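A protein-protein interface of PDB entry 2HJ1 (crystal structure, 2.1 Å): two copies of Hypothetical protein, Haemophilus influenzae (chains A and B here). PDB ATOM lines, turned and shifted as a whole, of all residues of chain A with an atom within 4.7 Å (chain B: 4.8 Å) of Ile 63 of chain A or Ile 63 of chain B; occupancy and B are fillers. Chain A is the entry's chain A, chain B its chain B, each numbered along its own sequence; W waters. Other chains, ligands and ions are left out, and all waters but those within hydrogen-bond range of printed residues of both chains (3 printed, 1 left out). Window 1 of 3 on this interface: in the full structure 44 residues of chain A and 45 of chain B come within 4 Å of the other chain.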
ATOM      1  N   VAL A  38      -1.343 -20.624  -9.819  1.00  0.00           N
ATOM      2  CA  VAL A  38      -2.483 -20.644 -10.739  1.00  0.00           C
ATOM      3  C   VAL A  38      -3.795 -20.416  -9.982  1.00  0.00           C
ATOM      4  O   VAL A  38      -4.656 -19.647 -10.419  1.00  0.00           O
ATOM      5  CB  VAL A  38      -2.572 -22.007 -11.485  1.00  0.00           C
ATOM      6  CG1 VAL A  38      -3.848 -22.086 -12.319  1.00  0.00           C
ATOM      7  CG2 VAL A  38      -1.280 -22.231 -12.313  1.00  0.00           C
ATOM      8  N   ILE A  61      -7.887 -27.482 -17.265  1.00  0.00           N
ATOM      9  CA  ILE A  61      -7.117 -26.268 -16.993  1.00  0.00           C
ATOM     10  C   ILE A  61      -5.679 -26.520 -17.366  1.00  0.00           C
ATOM     11  O   ILE A  61      -5.039 -27.450 -16.882  1.00  0.00           O
ATOM     12  CB  ILE A  61      -7.146 -25.798 -15.483  1.00  0.00           C
ATOM     13  CG1 ILE A  61      -8.596 -25.600 -14.999  1.00  0.00           C
ATOM     14  CG2 ILE A  61      -6.414 -24.431 -15.341  1.00  0.00           C
ATOM     15  CD1 ILE A  61      -8.727 -25.518 -13.440  1.00  0.00           C
ATOM     16  N   GLY A  62      -5.175 -25.703 -18.270  1.00  0.00           N
ATOM     17  CA  GLY A  62      -3.777 -25.807 -18.669  1.00  0.00           C
ATOM     18  C   GLY A  62      -3.154 -24.440 -18.714  1.00  0.00           C
ATOM     19  O   GLY A  62      -3.845 -23.425 -18.554  1.00  0.00           O
ATOM     20  N   ILE A  63      -1.841 -24.415 -18.888  1.00  0.00           N
ATOM     21  CA  ILE A  63      -1.092 -23.176 -18.827  1.00  0.00           C
ATOM     22  C   ILE A  63      -0.291 -23.124 -20.116  1.00  0.00           C
ATOM     23  O   ILE A  63       0.521 -24.018 -20.403  1.00  0.00           O
ATOM     24  CB  ILE A  63      -0.075 -23.211 -17.659  1.00  0.00           C
ATOM     25  CG1 ILE A  63      -0.727 -23.457 -16.278  1.00  0.00           C
ATOM     26  CG2 ILE A  63       0.870 -22.006 -17.639  1.00  0.00           C
ATOM     27  CD1 ILE A  63      -1.740 -22.445 -15.859  1.00  0.00           C
ATOM     28  N   PHE A  64      -0.484 -22.049 -20.869  1.00  0.00           N
ATOM     29  CA  PHE A  64       0.359 -21.805 -22.025  1.00  0.00           C
ATOM     30  C   PHE A  64       1.521 -20.881 -21.645  1.00  0.00           C
ATOM     31  O   PHE A  64       1.298 -19.793 -21.091  1.00  0.00           O
ATOM     32  CB  PHE A  64      -0.469 -21.194 -23.188  1.00  0.00           C
ATOM     33  CG  PHE A  64       0.395 -20.814 -24.366  1.00  0.00           C
ATOM     34  CD1 PHE A  64       0.927 -21.807 -25.192  1.00  0.00           C
ATOM     35  CD2 PHE A  64       0.746 -19.484 -24.596  1.00  0.00           C
ATOM     36  CE1 PHE A  64       1.767 -21.477 -26.255  1.00  0.00           C
ATOM     37  CE2 PHE A  64       1.578 -19.148 -25.672  1.00  0.00           C
ATOM     38  CZ  PHE A  64       2.094 -20.156 -26.489  1.00  0.00           C
ATOM     39  N   SER A  65       2.748 -21.312 -21.914  1.00  0.00           N
ATOM     40  CA  SER A  65       3.949 -20.527 -21.621  1.00  0.00           C
ATOM     41  C   SER A  65       4.745 -20.233 -22.921  1.00  0.00           C
ATOM     42  O   SER A  65       4.953 -21.139 -23.707  1.00  0.00           O
ATOM     43  CB  SER A  65       4.893 -21.301 -20.701  1.00  0.00           C
ATOM     44  OG  SER A  65       4.279 -21.536 -19.431  1.00  0.00           O
ATOM     45  N   ILE A  68       9.448 -20.397 -23.905  1.00  0.00           N
ATOM     46  CA  ILE A  68      10.383 -21.330 -23.310  1.00  0.00           C
ATOM     47  C   ILE A  68      11.843 -21.424 -23.610  1.00  0.00           C
ATOM     48  O   ILE A  68      12.342 -20.698 -24.452  1.00  0.00           O
ATOM     49  CB  ILE A  68       9.677 -22.743 -23.376  1.00  0.00           C
ATOM     50  CG1 ILE A  68       9.557 -23.282 -24.804  1.00  0.00           C
ATOM     51  CG2 ILE A  68       8.209 -22.600 -22.912  1.00  0.00           C
ATOM     52  CD1 ILE A  68      10.831 -23.939 -25.407  1.00  0.00           C
ATOM     53  N   LEU A  74      10.849 -31.625 -20.143  1.00  0.00           N
ATOM     54  CA  LEU A  74       9.436 -31.869 -20.444  1.00  0.00           C
ATOM     55  C   LEU A  74       8.741 -32.597 -19.290  1.00  0.00           C
ATOM     56  O   LEU A  74       9.351 -33.441 -18.636  1.00  0.00           O
ATOM     57  CB  LEU A  74       9.340 -32.694 -21.726  1.00  0.00           C
ATOM     58  CG  LEU A  74       9.713 -31.887 -22.985  1.00  0.00           C
ATOM     59  CD1 LEU A  74       9.867 -32.795 -24.222  1.00  0.00           C
ATOM     60  CD2 LEU A  74       8.692 -30.751 -23.243  1.00  0.00           C
ATOM     61  N   ASP A  78       3.063 -32.315 -21.739  1.00  0.00           N
ATOM     62  CA  ASP A  78       3.527 -31.045 -22.362  1.00  0.00           C
ATOM     63  C   ASP A  78       3.336 -31.098 -23.886  1.00  0.00           C
ATOM     64  O   ASP A  78       3.662 -32.088 -24.525  1.00  0.00           O
ATOM     65  CB  ASP A  78       5.005 -30.772 -22.043  1.00  0.00           C
ATOM     66  CG  ASP A  78       5.210 -30.049 -20.700  1.00  0.00           C
ATOM     67  OD1 ASP A  78       4.211 -29.592 -20.089  1.00  0.00           O
ATOM     68  OD2 ASP A  78       6.392 -29.913 -20.263  1.00  0.00           O
ATOM     69  N   ARG A  79       2.745 -30.046 -24.443  1.00  0.00           N
ATOM     70  CA  ARG A  79       2.694 -29.920 -25.883  1.00  0.00           C
ATOM     71  C   ARG A  79       3.643 -28.805 -26.323  1.00  0.00           C
ATOM     72  O   ARG A  79       3.428 -27.617 -26.018  1.00  0.00           O
ATOM     73  CB  ARG A  79       1.276 -29.645 -26.401  1.00  0.00           C
ATOM     74  CG  ARG A  79       1.251 -29.509 -27.908  1.00  0.00           C
ATOM     75  CD  ARG A  79      -0.150 -29.314 -28.442  1.00  0.00           C
ATOM     76  NE  ARG A  79      -0.761 -28.049 -27.996  1.00  0.00           N
ATOM     77  CZ  ARG A  79      -1.928 -27.948 -27.350  1.00  0.00           C
ATOM     78  NH1 ARG A  79      -2.633 -29.042 -27.031  1.00  0.00           N
ATOM     79  NH2 ARG A  79      -2.408 -26.743 -27.031  1.00  0.00           N
ATOM     80  N   ILE A  80       4.672 -29.192 -27.075  1.00  0.00           N
ATOM     81  CA  ILE A  80       5.604 -28.224 -27.671  1.00  0.00           C
ATOM     82  C   ILE A  80       4.989 -27.621 -28.909  1.00  0.00           C
ATOM     83  O   ILE A  80       4.660 -28.349 -29.828  1.00  0.00           O
ATOM     84  CB  ILE A  80       6.915 -28.884 -28.072  1.00  0.00           C
ATOM     85  CG1 ILE A  80       7.617 -29.491 -26.859  1.00  0.00           C
ATOM     86  CG2 ILE A  80       7.886 -27.797 -28.761  1.00  0.00           C
ATOM     87  CD1 ILE A  80       8.673 -30.550 -27.274  1.00  0.00           C
ATOM     88  N   VAL B  38      13.104 -30.111 -24.167  1.00  0.00           N
ATOM     89  CA  VAL B  38      12.486 -29.608 -25.404  1.00  0.00           C
ATOM     90  C   VAL B  38      13.344 -29.866 -26.658  1.00  0.00           C
ATOM     91  O   VAL B  38      12.873 -30.426 -27.636  1.00  0.00           O
ATOM     92  CB  VAL B  38      12.234 -28.116 -25.257  1.00  0.00           C
ATOM     93  CG1 VAL B  38      11.689 -27.522 -26.515  1.00  0.00           C
ATOM     94  CG2 VAL B  38      11.246 -27.856 -24.022  1.00  0.00           C
ATOM     95  N   ILE B  61       8.767 -20.688 -29.888  1.00  0.00           N
ATOM     96  CA  ILE B  61       8.294 -21.947 -29.293  1.00  0.00           C
ATOM     97  C   ILE B  61       7.548 -21.660 -27.965  1.00  0.00           C
ATOM     98  O   ILE B  61       8.102 -20.985 -27.073  1.00  0.00           O
ATOM     99  CB  ILE B  61       9.470 -22.920 -29.005  1.00  0.00           C
ATOM    100  CG1 ILE B  61      10.272 -23.180 -30.304  1.00  0.00           C
ATOM    101  CG2 ILE B  61       8.932 -24.259 -28.407  1.00  0.00           C
ATOM    102  CD1 ILE B  61      11.407 -24.101 -30.111  1.00  0.00           C
ATOM    103  N   GLY B  62       6.301 -22.140 -27.847  1.00  0.00           N
ATOM    104  CA  GLY B  62       5.645 -22.164 -26.542  1.00  0.00           C
ATOM    105  C   GLY B  62       5.391 -23.597 -26.084  1.00  0.00           C
ATOM    106  O   GLY B  62       5.652 -24.570 -26.837  1.00  0.00           O
ATOM    107  N   ILE B  63       4.879 -23.746 -24.865  1.00  0.00           N
ATOM    108  CA  ILE B  63       4.515 -25.088 -24.372  1.00  0.00           C
ATOM    109  C   ILE B  63       3.156 -24.954 -23.747  1.00  0.00           C
ATOM    110  O   ILE B  63       2.931 -24.046 -22.939  1.00  0.00           O
ATOM    111  CB  ILE B  63       5.525 -25.633 -23.380  1.00  0.00           C
ATOM    112  CG1 ILE B  63       6.768 -26.135 -24.135  1.00  0.00           C
ATOM    113  CG2 ILE B  63       4.977 -26.845 -22.588  1.00  0.00           C
ATOM    114  CD1 ILE B  63       7.936 -26.476 -23.229  1.00  0.00           C
ATOM    115  N   PHE B  64       2.232 -25.814 -24.162  1.00  0.00           N
ATOM    116  CA  PHE B  64       0.967 -25.965 -23.461  1.00  0.00           C
ATOM    117  C   PHE B  64       1.054 -27.132 -22.502  1.00  0.00           C
ATOM    118  O   PHE B  64       1.294 -28.287 -22.920  1.00  0.00           O
ATOM    119  CB  PHE B  64      -0.216 -26.160 -24.406  1.00  0.00           C
ATOM    120  CG  PHE B  64      -1.556 -26.124 -23.695  1.00  0.00           C
ATOM    121  CD1 PHE B  64      -2.030 -24.943 -23.148  1.00  0.00           C
ATOM    122  CD2 PHE B  64      -2.312 -27.260 -23.534  1.00  0.00           C
ATOM    123  CE1 PHE B  64      -3.239 -24.899 -22.484  1.00  0.00           C
ATOM    124  CE2 PHE B  64      -3.574 -27.222 -22.844  1.00  0.00           C
ATOM    125  CZ  PHE B  64      -4.016 -26.034 -22.335  1.00  0.00           C
ATOM    126  N   SER B  65       0.857 -26.830 -21.215  1.00  0.00           N
ATOM    127  CA  SER B  65       0.992 -27.818 -20.138  1.00  0.00           C
ATOM    128  C   SER B  65      -0.397 -28.153 -19.568  1.00  0.00           C
ATOM    129  O   SER B  65      -1.178 -27.247 -19.261  1.00  0.00           O
ATOM    130  CB  SER B  65       1.821 -27.241 -18.996  1.00  0.00           C
ATOM    131  OG  SER B  65       3.187 -27.076 -19.353  1.00  0.00           O
ATOM    132  N   ILE B  68      -2.129 -29.624 -14.778  1.00  0.00           N
ATOM    133  CA  ILE B  68      -1.160 -28.951 -13.929  1.00  0.00           C
ATOM    134  C   ILE B  68      -1.720 -29.020 -12.494  1.00  0.00           C
ATOM    135  O   ILE B  68      -2.900 -29.321 -12.288  1.00  0.00           O
ATOM    136  CB  ILE B  68      -1.049 -27.475 -14.362  1.00  0.00           C
ATOM    137  CG1 ILE B  68      -2.466 -26.882 -14.478  1.00  0.00           C
ATOM    138  CG2 ILE B  68      -0.304 -27.391 -15.719  1.00  0.00           C
ATOM    139  CD1 ILE B  68      -2.646 -25.569 -13.949  1.00  0.00           C
ATOM    140  N   LEU B  74       2.997 -19.063 -11.479  1.00  0.00           N
ATOM    141  CA  LEU B  74       2.916 -18.457 -12.814  1.00  0.00           C
ATOM    142  C   LEU B  74       4.166 -17.655 -13.164  1.00  0.00           C
ATOM    143  O   LEU B  74       4.872 -17.174 -12.269  1.00  0.00           O
ATOM    144  CB  LEU B  74       1.692 -17.561 -12.941  1.00  0.00           C
ATOM    145  CG  LEU B  74       0.388 -18.362 -12.941  1.00  0.00           C
ATOM    146  CD1 LEU B  74      -0.694 -17.426 -12.496  1.00  0.00           C
ATOM    147  CD2 LEU B  74       0.069 -18.929 -14.325  1.00  0.00           C
ATOM    148  N   ASP B  78       2.325 -16.078 -19.042  1.00  0.00           N
ATOM    149  CA  ASP B  78       1.512 -17.306 -18.939  1.00  0.00           C
ATOM    150  C   ASP B  78       0.050 -17.002 -19.223  1.00  0.00           C
ATOM    151  O   ASP B  78      -0.463 -15.945 -18.848  1.00  0.00           O
ATOM    152  CB  ASP B  78       1.650 -17.974 -17.582  1.00  0.00           C
ATOM    153  CG  ASP B  78       2.894 -18.843 -17.475  1.00  0.00           C
ATOM    154  OD1 ASP B  78       3.598 -19.116 -18.494  1.00  0.00           O
ATOM    155  OD2 ASP B  78       3.195 -19.265 -16.334  1.00  0.00           O
ATOM    156  N   ARG B  79      -0.606 -17.916 -19.928  1.00  0.00           N
ATOM    157  CA  ARG B  79      -2.050 -17.878 -20.046  1.00  0.00           C
ATOM    158  C   ARG B  79      -2.632 -19.159 -19.460  1.00  0.00           C
ATOM    159  O   ARG B  79      -2.217 -20.256 -19.834  1.00  0.00           O
ATOM    160  CB  ARG B  79      -2.497 -17.755 -21.493  1.00  0.00           C
ATOM    161  CG  ARG B  79      -4.008 -17.651 -21.596  1.00  0.00           C
ATOM    162  CD  ARG B  79      -4.469 -17.832 -23.041  1.00  0.00           C
ATOM    163  NE  ARG B  79      -4.319 -16.602 -23.812  1.00  0.00           N
ATOM    164  CZ  ARG B  79      -4.704 -16.437 -25.081  1.00  0.00           C
ATOM    165  NH1 ARG B  79      -4.512 -15.258 -25.686  1.00  0.00           N
ATOM    166  NH2 ARG B  79      -5.287 -17.434 -25.748  1.00  0.00           N
ATOM    167  N   ILE B  80      -3.602 -18.987 -18.574  1.00  0.00           N
ATOM    168  CA  ILE B  80      -4.365 -20.068 -17.980  1.00  0.00           C
ATOM    169  C   ILE B  80      -5.563 -20.278 -18.877  1.00  0.00           C
ATOM    170  O   ILE B  80      -6.349 -19.342 -19.119  1.00  0.00           O
ATOM    171  CB  ILE B  80      -4.855 -19.659 -16.553  1.00  0.00           C
ATOM    172  CG1 ILE B  80      -3.664 -19.347 -15.630  1.00  0.00           C
ATOM    173  CG2 ILE B  80      -5.858 -20.697 -15.988  1.00  0.00           C
ATOM    174  CD1 ILE B  80      -4.043 -18.637 -14.338  1.00  0.00           C
HETATM  175  O   HOH W   1       3.481 -24.301 -19.764  1.00  0.00           O
HETATM  176  O   HOH W   2      -5.013 -29.183 -14.943  1.00  0.00           O
HETATM  177  O   HOH W   3       6.131 -27.977 -18.218  1.00  0.00           O
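Along chain A the printed residues that touch a printed residue of chain B span positions 38 to 80. Of the 11 printed residues of chain B, 10 touch a printed residue of chain A.
Ile 63 of chain A touches just these residues of chain B: Ile 63 (3.5 Å), Phe 64 (3.7 Å), Ser 65 (2.9 Å), Ile 68 (3.7 Å), Asp 78 (3.8 Å), Arg 79 (3.3 Å) and Ile 80 (3.7 Å). Ile 63 of chain B touches six residues of chain A. Printed residues of chain A within 4 Å of Ile 80 of chain B: Ile 61, Gly 62 and Ile 63. Of the printed residues of chain A, Asp 78 of chain B touches Ile 63 (3.8 Å), Phe 64 (3.3 Å) and Ser 65 (2.7 Å). Of the printed residues of chain A, Arg 79 of chain B touches Gly 62 (3.8 Å), Ile 63 (3.3 Å) and Phe 64 (2.7 Å). Printed residues of chain B within 4 Å of Val 38 of chain A: Ile 68. The nearest printed residue of chain A that does not touch Ser 65 of chain B is Ile 61 of chain A (4.5 Å).
Ile 61 of chain A touches Ile 80 of chain B, and with the chains exchanged Ile 80 of chain A touches Ile 61 of chain B. Ile 63 of chain A touches Ser 65 of chain B, and with the chains exchanged Ser 65 of chain A touches Ile 63 of chain B. Phe 64 of chain A touches Arg 79 of chain B, and with the chains exchanged Arg 79 of chain A touches Phe 64 of chain B. Leu 74 of chain A touches Val 38 of chain B, but with the chains exchanged Val 38 of chain A does not touch Leu 74 of chain B (4.1 Å). Positions printed for both chains: 38, 61, 62, 63, 64, 65, 68, 74, 78, 79 and 80. Of the 34 pairs that touch across the chains among the printed residues, 32 have their exchanged pair printed and touching as well.
The backbone carbonyl oxygen of Ile 63 of chain A lies close to the backbone carbonyl oxygen of Ile 63 of chain B (3.5 Å). The side-chain carboxylate (OD1) of Asp 78 of chain A is in hydrogen-bond range of the side-chain hydroxyl (OG) of Ser 65 of chain B (2.8 Å). O of Phe 64 of chain B sits at hydrogen-bond distance from N of Arg 79 of chain A, 2.7 Å away. The backbone NH of Ile 63 of chain B is in hydrogen-bond range of the backbone carbonyl oxygen of Ser 65 of chain A. N of Ile 63 of chain A is in hydrogen-bond range of O of Ser 65 of chain B (2.9 Å). The backbone carbonyl oxygen (O) of Ile 61 of chain B sits at hydrogen-bond distance from the backbone NH (N) of Ile 68 of chain A. The side-chain hydroxyl (OG) of Ser 65 of chain A sits at hydrogen-bond distance from the side-chain carboxylate (OD1) of Asp 78 of chain B, at 2.7 Å. The backbone carbonyl oxygen (O) of Arg 79 of chain B sits at hydrogen-bond distance from the backbone NH (N) of Phe 64 of chain A (2.7 Å).
Among the printed residues, merely in contact across the chains: Gly 62 of chain A with Ser 65 of chain B (3.0 Å), Ser 65 of chain A with Gly 62 of chain B (3.1 Å), Arg 79 of chain A with Ile 63 of chain B (3.2 Å), Ile 63 of chain A with Arg 79 of chain B (3.3 Å), Phe 64 of chain A with Asp 78 of chain B (3.3 Å), Gly 62 of chain A with Ile 80 of chain B (3.4 Å), Phe 64 of chain A with Ile 63 of chain B (3.5 Å), Ile 61 of chain A with Ile 68 of chain B (3.6 Å), Asp 78 of chain A with Phe 64 of chain B (3.6 Å), Ile 63 of chain A with Phe 64 of chain B (3.7 Å), Ile 63 of chain A with Ile 80 of chain B (3.7 Å), Gly 62 of chain A with Phe 64 of chain B (3.7 Å), Ile 63 of chain A with Ile 68 of chain B (3.7 Å), Ile 80 of chain A with Ile 61 of chain B (3.7 Å), Asp 78 of chain A with Ile 63 of chain B (3.7 Å), Ile 80 of chain A with Gly 62 of chain B (3.7 Å), Ile 63 of chain A with Asp 78 of chain B (3.8 Å), Gly 62 of chain A with Arg 79 of chain B (3.8 Å), Ile 61 of chain A with Ile 80 of chain B (3.8 Å), Ile 68 of chain A with Val 38 of chain B (3.8 Å), Arg 79 of chain A with Gly 62 of chain B (3.9 Å), Ile 68 of chain A with Ile 63 of chain B (3.9 Å), Leu 74 of chain A with Val 38 of chain B (3.9 Å), Phe 64 of chain A with Gly 62 of chain B (3.9 Å), Val 38 of chain A with Ile 68 of chain B (3.96 Å) and Phe 64 of chain A with Phe 64 of chain B (3.99 Å).
Water W2 lies within hydrogen-bond range of O of Ile 61 of chain A and N of Ile 68 of chain B. Water W1 lies within hydrogen-bond range of OG of Ser 65 of chain B, OG of Ser 65 of chain A, O of Ile 63 of chain A and O of Ile 63 of chain B. Water W3 bridges OD2 of Asp 78 of chain A and OG of Ser 65 of chain B.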
